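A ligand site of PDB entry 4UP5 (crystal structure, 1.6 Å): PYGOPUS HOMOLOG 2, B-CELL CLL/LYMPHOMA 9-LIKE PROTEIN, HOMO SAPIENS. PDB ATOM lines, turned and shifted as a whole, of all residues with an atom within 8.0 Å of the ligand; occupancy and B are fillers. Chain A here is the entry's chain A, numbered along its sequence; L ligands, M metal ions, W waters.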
ATOM      1  N   CYS A   5     -27.883  20.527   9.966  1.00  0.00           N
ATOM      2  CA  CYS A   5     -27.835  19.095   9.755  1.00  0.00           C
ATOM      3  C   CYS A   5     -26.864  18.445  10.724  1.00  0.00           C
ATOM      4  O   CYS A   5     -25.680  18.884  10.849  1.00  0.00           O
ATOM      5  CB  CYS A   5     -27.428  18.797   8.283  1.00  0.00           C
ATOM      6  SG  CYS A   5     -27.182  17.047   7.925  1.00  0.00           S
ATOM      7  N   GLY A   6     -27.311  17.369  11.397  1.00  0.00           N
ATOM      8  CA  GLY A   6     -26.497  16.555  12.254  1.00  0.00           C
ATOM      9  C   GLY A   6     -25.225  15.995  11.692  1.00  0.00           C
ATOM     10  O   GLY A   6     -24.276  15.661  12.417  1.00  0.00           O
ATOM     11  N   ALA A   7     -25.228  15.803  10.377  1.00  0.00           N
ATOM     12  CA  ALA A   7     -24.073  15.286   9.705  1.00  0.00           C
ATOM     13  C   ALA A   7     -23.194  16.310   9.101  1.00  0.00           C
ATOM     14  O   ALA A   7     -21.999  16.387   9.419  1.00  0.00           O
ATOM     15  CB  ALA A   7     -24.539  14.300   8.643  1.00  0.00           C
ATOM     16  N   CYS A   8     -23.714  17.205   8.272  1.00  0.00           N
ATOM     17  CA  CYS A   8     -22.825  18.055   7.546  1.00  0.00           C
ATOM     18  C   CYS A   8     -22.661  19.452   8.201  1.00  0.00           C
ATOM     19  O   CYS A   8     -21.864  20.305   7.768  1.00  0.00           O
ATOM     20  CB  CYS A   8     -23.383  18.257   6.143  1.00  0.00           C
ATOM     21  SG  CYS A   8     -24.844  19.233   5.900  1.00  0.00           S
ATOM     22  N   ARG A   9     -23.542  19.684   9.145  1.00  0.00           N
ATOM     23  CA  ARG A   9     -23.602  20.979   9.884  1.00  0.00           C
ATOM     24  C   ARG A   9     -24.102  22.212   9.179  1.00  0.00           C
ATOM     25  O   ARG A   9     -24.013  23.295   9.784  1.00  0.00           O
ATOM     26  CB  ARG A   9     -22.279  21.259  10.510  1.00  0.00           C
ATOM     27  CG  ARG A   9     -21.815  20.141  11.443  1.00  0.00           C
ATOM     28  CD  ARG A   9     -22.782  19.833  12.546  1.00  0.00           C
ATOM     29  NE  ARG A   9     -22.006  19.215  13.631  1.00  0.00           N
ATOM     30  CZ  ARG A   9     -22.495  18.584  14.687  1.00  0.00           C
ATOM     31  NH1 ARG A   9     -23.816  18.459  14.858  1.00  0.00           N
ATOM     32  NH2 ARG A   9     -21.622  18.069  15.576  1.00  0.00           N
ATOM     33  N   ILE A  19     -34.806  14.371   7.899  1.00  0.00           N
ATOM     34  CA  ILE A  19     -35.328  13.411   8.890  1.00  0.00           C
ATOM     35  C   ILE A  19     -34.797  13.804  10.278  1.00  0.00           C
ATOM     36  O   ILE A  19     -33.694  14.231  10.453  1.00  0.00           O
ATOM     37  CB  ILE A  19     -35.028  11.968   8.428  1.00  0.00           C
ATOM     38  CG1 ILE A  19     -35.697  10.972   9.357  1.00  0.00           C
ATOM     39  CG2 ILE A  19     -33.558  11.715   8.348  1.00  0.00           C
ATOM     40  CD1 ILE A  19     -36.425   9.938   8.570  1.00  0.00           C
ATOM     41  N   CYS A  21     -33.798  12.715  14.164  1.00  0.00           N
ATOM     42  CA  CYS A  21     -33.371  11.649  15.019  1.00  0.00           C
ATOM     43  C   CYS A  21     -34.219  11.660  16.309  1.00  0.00           C
ATOM     44  O   CYS A  21     -33.922  12.361  17.246  1.00  0.00           O
ATOM     45  CB  CYS A  21     -31.918  11.684  15.352  1.00  0.00           C
ATOM     46  SG  CYS A  21     -31.384  10.313  16.433  1.00  0.00           S
ATOM     47  N   CYS A  25     -31.065  12.117  19.854  1.00  0.00           N
ATOM     48  CA  CYS A  25     -30.386  13.418  19.902  1.00  0.00           C
ATOM     49  C   CYS A  25     -31.263  14.595  19.437  1.00  0.00           C
ATOM     50  O   CYS A  25     -30.918  15.780  19.670  1.00  0.00           O
ATOM     51  CB  CYS A  25     -29.070  13.381  19.121  1.00  0.00           C
ATOM     52  SG  CYS A  25     -29.307  13.270  17.278  1.00  0.00           S
ATOM     53  N   LYS A  27     -31.691  15.789  16.642  1.00  0.00           N
ATOM     54  CA  LYS A  27     -31.139  16.601  15.534  1.00  0.00           C
ATOM     55  C   LYS A  27     -31.737  16.230  14.199  1.00  0.00           C
ATOM     56  O   LYS A  27     -32.084  15.052  13.995  1.00  0.00           O
ATOM     57  CB  LYS A  27     -29.644  16.440  15.423  1.00  0.00           C
ATOM     58  CG  LYS A  27     -28.956  17.088  16.602  1.00  0.00           C
ATOM     59  CD  LYS A  27     -27.504  16.799  16.727  1.00  0.00           C
ATOM     60  CE  LYS A  27     -27.047  17.408  18.057  1.00  0.00           C
ATOM     61  NZ  LYS A  27     -25.618  17.782  18.016  1.00  0.00           N
ATOM     62  N   PHE A  29     -31.500  15.920  10.059  1.00  0.00           N
ATOM     63  CA  PHE A  29     -30.451  15.602   9.125  1.00  0.00           C
ATOM     64  C   PHE A  29     -30.995  15.716   7.683  1.00  0.00           C
ATOM     65  O   PHE A  29     -32.156  15.330   7.392  1.00  0.00           O
ATOM     66  CB  PHE A  29     -30.010  14.134   9.297  1.00  0.00           C
ATOM     67  CG  PHE A  29     -29.178  13.855  10.517  1.00  0.00           C
ATOM     68  CD1 PHE A  29     -29.761  13.883  11.756  1.00  0.00           C
ATOM     69  CD2 PHE A  29     -27.857  13.473  10.389  1.00  0.00           C
ATOM     70  CE1 PHE A  29     -29.007  13.604  12.890  1.00  0.00           C
ATOM     71  CE2 PHE A  29     -27.090  13.211  11.509  1.00  0.00           C
ATOM     72  CZ  PHE A  29     -27.737  13.251  12.761  1.00  0.00           C
ATOM     73  N   HIS A  30     -30.171  16.150   6.736  1.00  0.00           N
ATOM     74  CA  HIS A  30     -30.590  15.981   5.341  1.00  0.00           C
ATOM     75  C   HIS A  30     -30.688  14.563   5.025  1.00  0.00           C
ATOM     76  O   HIS A  30     -29.757  13.837   5.299  1.00  0.00           O
ATOM     77  CB  HIS A  30     -29.506  16.588   4.397  1.00  0.00           C
ATOM     78  CG  HIS A  30     -29.321  18.053   4.562  1.00  0.00           C
ATOM     79  ND1 HIS A  30     -28.146  18.604   5.061  1.00  0.00           N
ATOM     80  CD2 HIS A  30     -30.119  19.095   4.217  1.00  0.00           C
ATOM     81  CE1 HIS A  30     -28.266  19.940   5.002  1.00  0.00           C
ATOM     82  NE2 HIS A  30     -29.447  20.252   4.537  1.00  0.00           N
ATOM     83  N   ARG A  31     -31.748  14.124   4.329  1.00  0.00           N
ATOM     84  CA  ARG A  31     -31.842  12.760   3.897  1.00  0.00           C
ATOM     85  C   ARG A  31     -30.552  12.335   3.128  1.00  0.00           C
ATOM     86  O   ARG A  31     -29.936  11.296   3.409  1.00  0.00           O
ATOM     87  CB  ARG A  31     -33.063  12.563   2.999  1.00  0.00           C
ATOM     88  CG  ARG A  31     -33.156  11.122   2.462  1.00  0.00           C
ATOM     89  CD  ARG A  31     -34.113  11.007   1.280  1.00  0.00           C
ATOM     90  NE  ARG A  31     -33.748  11.727   0.081  1.00  0.00           N
ATOM     91  CZ  ARG A  31     -32.804  11.329  -0.736  1.00  0.00           C
ATOM     92  NH1 ARG A  31     -32.130  10.196  -0.572  1.00  0.00           N
ATOM     93  NH2 ARG A  31     -32.531  12.086  -1.815  1.00  0.00           N
ATOM     94  N   GLU A  32     -30.072  13.176   2.194  1.00  0.00           N
ATOM     95  CA  GLU A  32     -28.874  12.787   1.410  1.00  0.00           C
ATOM     96  C   GLU A  32     -27.602  12.688   2.220  1.00  0.00           C
ATOM     97  O   GLU A  32     -26.725  11.905   1.897  1.00  0.00           O
ATOM     98  CB  GLU A  32     -28.633  13.788   0.280  1.00  0.00           C
ATOM     99  CG  GLU A  32     -29.760  13.761  -0.779  1.00  0.00           C
ATOM    100  CD  GLU A  32     -29.638  14.871  -1.862  1.00  0.00           C
ATOM    101  OE1 GLU A  32     -28.587  15.571  -1.891  1.00  0.00           O
ATOM    102  OE2 GLU A  32     -30.585  15.052  -2.662  1.00  0.00           O
ATOM    103  N   CYS A  33     -27.504  13.363   3.369  1.00  0.00           N
ATOM    104  CA  CYS A  33     -26.350  13.113   4.199  1.00  0.00           C
ATOM    105  C   CYS A  33     -26.281  11.794   4.983  1.00  0.00           C
ATOM    106  O   CYS A  33     -25.294  11.404   5.641  1.00  0.00           O
ATOM    107  CB  CYS A  33     -26.281  14.322   5.163  1.00  0.00           C
ATOM    108  SG  CYS A  33     -25.838  15.890   4.317  1.00  0.00           S
ATOM    109  N   THR A  34     -27.404  11.122   5.053  1.00  0.00           N
ATOM    110  CA  THR A  34     -27.509   9.942   5.854  1.00  0.00           C
ATOM    111  C   THR A  34     -27.280   8.685   5.053  1.00  0.00           C
ATOM    112  O   THR A  34     -27.011   7.645   5.615  1.00  0.00           O
ATOM    113  CB  THR A  34     -28.888   9.767   6.488  1.00  0.00           C
ATOM    114  OG1 THR A  34     -29.886   9.587   5.464  1.00  0.00           O
ATOM    115  CG2 THR A  34     -29.202  11.083   7.383  1.00  0.00           C
ATOM    116  N   GLY A  35     -27.444   8.764   3.724  1.00  0.00           N
ATOM    117  CA  GLY A  35     -27.486   7.590   2.908  1.00  0.00           C
ATOM    118  C   GLY A  35     -28.776   6.857   2.788  1.00  0.00           C
ATOM    119  O   GLY A  35     -28.878   5.894   2.040  1.00  0.00           O
ATOM    120  N   MET A  36     -29.833   7.416   3.393  1.00  0.00           N
ATOM    121  CA  MET A  36     -31.162   6.869   3.287  1.00  0.00           C
ATOM    122  C   MET A  36     -31.658   7.010   1.789  1.00  0.00           C
ATOM    123  O   MET A  36     -31.560   8.077   1.202  1.00  0.00           O
ATOM    124  CB  MET A  36     -32.091   7.630   4.201  1.00  0.00           C
ATOM    125  CG  MET A  36     -33.435   6.993   4.239  1.00  0.00           C
ATOM    126  SD  MET A  36     -34.518   7.787   5.477  1.00  0.00           S
ATOM    127  CE  MET A  36     -33.545   7.356   7.001  1.00  0.00           C
ATOM    128  N   TRP A  52     -36.604   7.222  13.543  1.00  0.00           N
ATOM    129  CA  TRP A  52     -35.285   7.052  12.970  1.00  0.00           C
ATOM    130  C   TRP A  52     -34.238   7.389  14.020  1.00  0.00           C
ATOM    131  O   TRP A  52     -34.461   8.300  14.824  1.00  0.00           O
ATOM    132  CB  TRP A  52     -35.179   7.948  11.723  1.00  0.00           C
ATOM    133  CG  TRP A  52     -33.858   7.889  11.112  1.00  0.00           C
ATOM    134  CD1 TRP A  52     -33.342   6.869  10.393  1.00  0.00           C
ATOM    135  CD2 TRP A  52     -32.887   8.927  11.128  1.00  0.00           C
ATOM    136  NE1 TRP A  52     -32.050   7.165   9.992  1.00  0.00           N
ATOM    137  CE2 TRP A  52     -31.755   8.428  10.440  1.00  0.00           C
ATOM    138  CE3 TRP A  52     -32.824  10.227  11.698  1.00  0.00           C
ATOM    139  CZ2 TRP A  52     -30.579   9.209  10.253  1.00  0.00           C
ATOM    140  CZ3 TRP A  52     -31.703  10.966  11.529  1.00  0.00           C
ATOM    141  CH2 TRP A  52     -30.566  10.456  10.833  1.00  0.00           C
ATOM    142  N   ALA A  53     -33.171   6.611  14.026  1.00  0.00           N
ATOM    143  CA  ALA A  53     -32.000   6.858  14.827  1.00  0.00           C
ATOM    144  C   ALA A  53     -30.808   7.114  13.945  1.00  0.00           C
ATOM    145  O   ALA A  53     -30.527   6.323  13.012  1.00  0.00           O
ATOM    146  CB  ALA A  53     -31.726   5.634  15.671  1.00  0.00           C
ATOM    147  N   CYS A  54     -30.083   8.196  14.225  1.00  0.00           N
ATOM    148  CA  CYS A  54     -28.861   8.490  13.542  1.00  0.00           C
ATOM    149  C   CYS A  54     -27.731   7.587  13.954  1.00  0.00           C
ATOM    150  O   CYS A  54     -27.893   6.826  14.948  1.00  0.00           O
ATOM    151  CB  CYS A  54     -28.480   9.948  13.637  1.00  0.00           C
ATOM    152  SG  CYS A  54     -27.676  10.309  15.256  1.00  0.00           S
ATOM    153  N   ASP A  55     -26.660   7.588  13.159  1.00  0.00           N
ATOM    154  CA  ASP A  55     -25.497   6.681  13.399  1.00  0.00           C
ATOM    155  C   ASP A  55     -24.863   6.862  14.794  1.00  0.00           C
ATOM    156  O   ASP A  55     -24.230   5.946  15.304  1.00  0.00           O
ATOM    157  CB  ASP A  55     -24.443   6.846  12.325  1.00  0.00           C
ATOM    158  CG  ASP A  55     -24.834   6.206  10.996  1.00  0.00           C
ATOM    159  OD1 ASP A  55     -25.849   5.402  10.878  1.00  0.00           O
ATOM    160  OD2 ASP A  55     -24.112   6.537  10.038  1.00  0.00           O
ATOM    161  N   LEU A  56     -25.073   8.019  15.414  1.00  0.00           N
ATOM    162  CA  LEU A  56     -24.576   8.246  16.759  1.00  0.00           C
ATOM    163  C   LEU A  56     -25.518   7.770  17.812  1.00  0.00           C
ATOM    164  O   LEU A  56     -25.063   7.353  18.850  1.00  0.00           O
ATOM    165  CB  LEU A  56     -24.229   9.712  16.912  1.00  0.00           C
ATOM    166  CG  LEU A  56     -23.116  10.192  15.970  1.00  0.00           C
ATOM    167  CD1 LEU A  56     -22.748  11.617  16.362  1.00  0.00           C
ATOM    168  CD2 LEU A  56     -21.885   9.284  16.059  1.00  0.00           C
ATOM    169  N   CYS A  57     -26.806   7.705  17.569  1.00  0.00           N
ATOM    170  CA  CYS A  57     -27.737   7.328  18.609  1.00  0.00           C
ATOM    171  C   CYS A  57     -28.068   5.800  18.626  1.00  0.00           C
ATOM    172  O   CYS A  57     -27.492   5.024  17.830  1.00  0.00           O
ATOM    173  CB  CYS A  57     -28.950   8.179  18.494  1.00  0.00           C
ATOM    174  SG  CYS A  57     -28.530   9.908  18.865  1.00  0.00           S
ATOM    175  N   THR A  75     -32.389   2.480  12.110  1.00  0.00           N
ATOM    176  CA  THR A  75     -31.225   3.116  11.607  1.00  0.00           C
ATOM    177  C   THR A  75     -31.439   3.272  10.102  1.00  0.00           C
ATOM    178  O   THR A  75     -32.407   2.699   9.548  1.00  0.00           O
ATOM    179  CB  THR A  75     -30.004   2.243  11.800  1.00  0.00           C
ATOM    180  OG1 THR A  75     -30.193   0.984  11.131  1.00  0.00           O
ATOM    181  CG2 THR A  75     -29.836   1.985  13.297  1.00  0.00           C
ATOM    182  N   THR A  76     -30.544   4.056   9.516  1.00  0.00           N
ATOM    183  CA  THR A  76     -30.581   4.234   8.046  1.00  0.00           C
ATOM    184  C   THR A  76     -30.500   2.886   7.331  1.00  0.00           C
ATOM    185  O   THR A  76     -31.265   2.564   6.407  1.00  0.00           O
ATOM    186  CB  THR A  76     -29.495   5.187   7.595  1.00  0.00           C
ATOM    187  OG1 THR A  76     -29.762   6.421   8.224  1.00  0.00           O
ATOM    188  CG2 THR A  76     -29.502   5.304   6.059  1.00  0.00           C
ATOM    189  N   HIS A  77     -29.513   2.097   7.686  1.00  0.00           N
ATOM    190  CA  HIS A  77     -29.322   0.896   6.952  1.00  0.00           C
ATOM    191  C   HIS A  77     -30.465  -0.043   7.108  1.00  0.00           C
ATOM    192  O   HIS A  77     -30.896  -0.685   6.117  1.00  0.00           O
ATOM    193  CB  HIS A  77     -28.014   0.241   7.344  1.00  0.00           C
ATOM    194  CG  HIS A  77     -26.854   1.007   6.881  1.00  0.00           C
ATOM    195  ND1 HIS A  77     -25.566   0.783   7.300  1.00  0.00           N
ATOM    196  CD2 HIS A  77     -26.793   2.054   6.007  1.00  0.00           C
ATOM    197  CE1 HIS A  77     -24.763   1.641   6.701  1.00  0.00           C
ATOM    198  NE2 HIS A  77     -25.484   2.433   5.948  1.00  0.00           N
HETATM  199  C1  LIG L   1     -22.882  11.727  11.230  1.00  0.00           C
HETATM  200  O1  LIG L   1     -21.757  12.518  11.317  1.00  0.00           O
HETATM  201  C2  LIG L   1     -21.480  13.384  10.232  1.00  0.00           C
HETATM  202  C3  LIG L   1     -23.176  11.100  10.038  1.00  0.00           C
HETATM  203  C4  LIG L   1     -24.316  10.321   9.979  1.00  0.00           C
HETATM  204  C5  LIG L   1     -25.161  10.161  11.084  1.00  0.00           C
HETATM  205  C6  LIG L   1     -24.833  10.808  12.274  1.00  0.00           C
HETATM  206  C7  LIG L   1     -23.693  11.590  12.342  1.00  0.00           C
HETATM  207  N1  LIG L   1     -26.265   9.338  10.883  1.00  0.00           N
HETATM  208  C8  LIG L   1     -26.281   8.885   9.653  1.00  0.00           C
HETATM  209  N2  LIG L   1     -27.223   8.080   9.157  1.00  0.00           N
HETATM  210  S1  LIG L   1     -24.944   9.408   8.631  1.00  0.00           S
HETATM  211 ZN    ZN M   1     -29.225  10.955  16.946  1.00  0.00          ZN
HETATM  212 ZN    ZN M   2     -26.472  17.584   5.708  1.00  0.00          ZN
HETATM  213  O   HOH W   1     -28.746   5.627  11.109  1.00  0.00           O
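N of Ala 7 sits close to SG of Cys 5 (3.4 Å). The side-chain hydroxyl of Thr 76 lies within hydrogen-bond range of the indole nitrogen of Trp 52, 3.0 Å away. O of Ile 19 sits at hydrogen-bond distance from N of Phe 29. N of Met 36 is in hydrogen-bond range of OG1 of Thr 34. OG1 of Thr 34 lies within hydrogen-bond range of O of Arg 31 (2.7 Å). SG of Cys 54 lies close to N of Leu 56 (3.5 Å).
Water W1 lies within hydrogen-bond range of the backbone carbonyl oxygen (O) of Ala 53, the backbone NH (N) of Thr 76, the side-chain carboxylate (OD1) of Asp 55 and a nitrogen (N2) of the ligand.
N1 of the ligand lies within hydrogen-bond range of N of Asp 55, 2.9 Å away. OD1 of Asp 55 lies within hydrogen-bond range of N2 of the ligand (3.5 Å). A nitrogen (N2) of the ligand lies within hydrogen-bond range of the side-chain hydroxyl (OG1) of Thr 76, 3.2 Å away.
A sulfur (S1) of the ligand sits close to the backbone carbonyl oxygen of Cys 33, at 3.6 Å. Ala 7 touches the ligand (O to C2, 3.2 Å). Phe 29 touches the ligand (CE2 to C6, 3.4 Å). Thr 34 touches the ligand (CB to N2, 3.6 Å). CZ2 of Trp 52 touches N2 of the ligand, at 3.7 Å. Cys 54 touches the ligand (CB to N1, 3.6 Å). CG of Leu 56 touches C7 of the ligand, at 3.9 Å. Hydrophobic or aromatic side chains within 4 Å of the ligand: Ala 7, Phe 29, Trp 52 and Leu 56. Within 4 Å of the ligand: Ala 7, Phe 29, Cys 33, Thr 34, Trp 52, Cys 54, Asp 55, Leu 56 and Thr 76. The nearest printed residue that does not touch the ligand is Gly 6 (4.1 Å).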
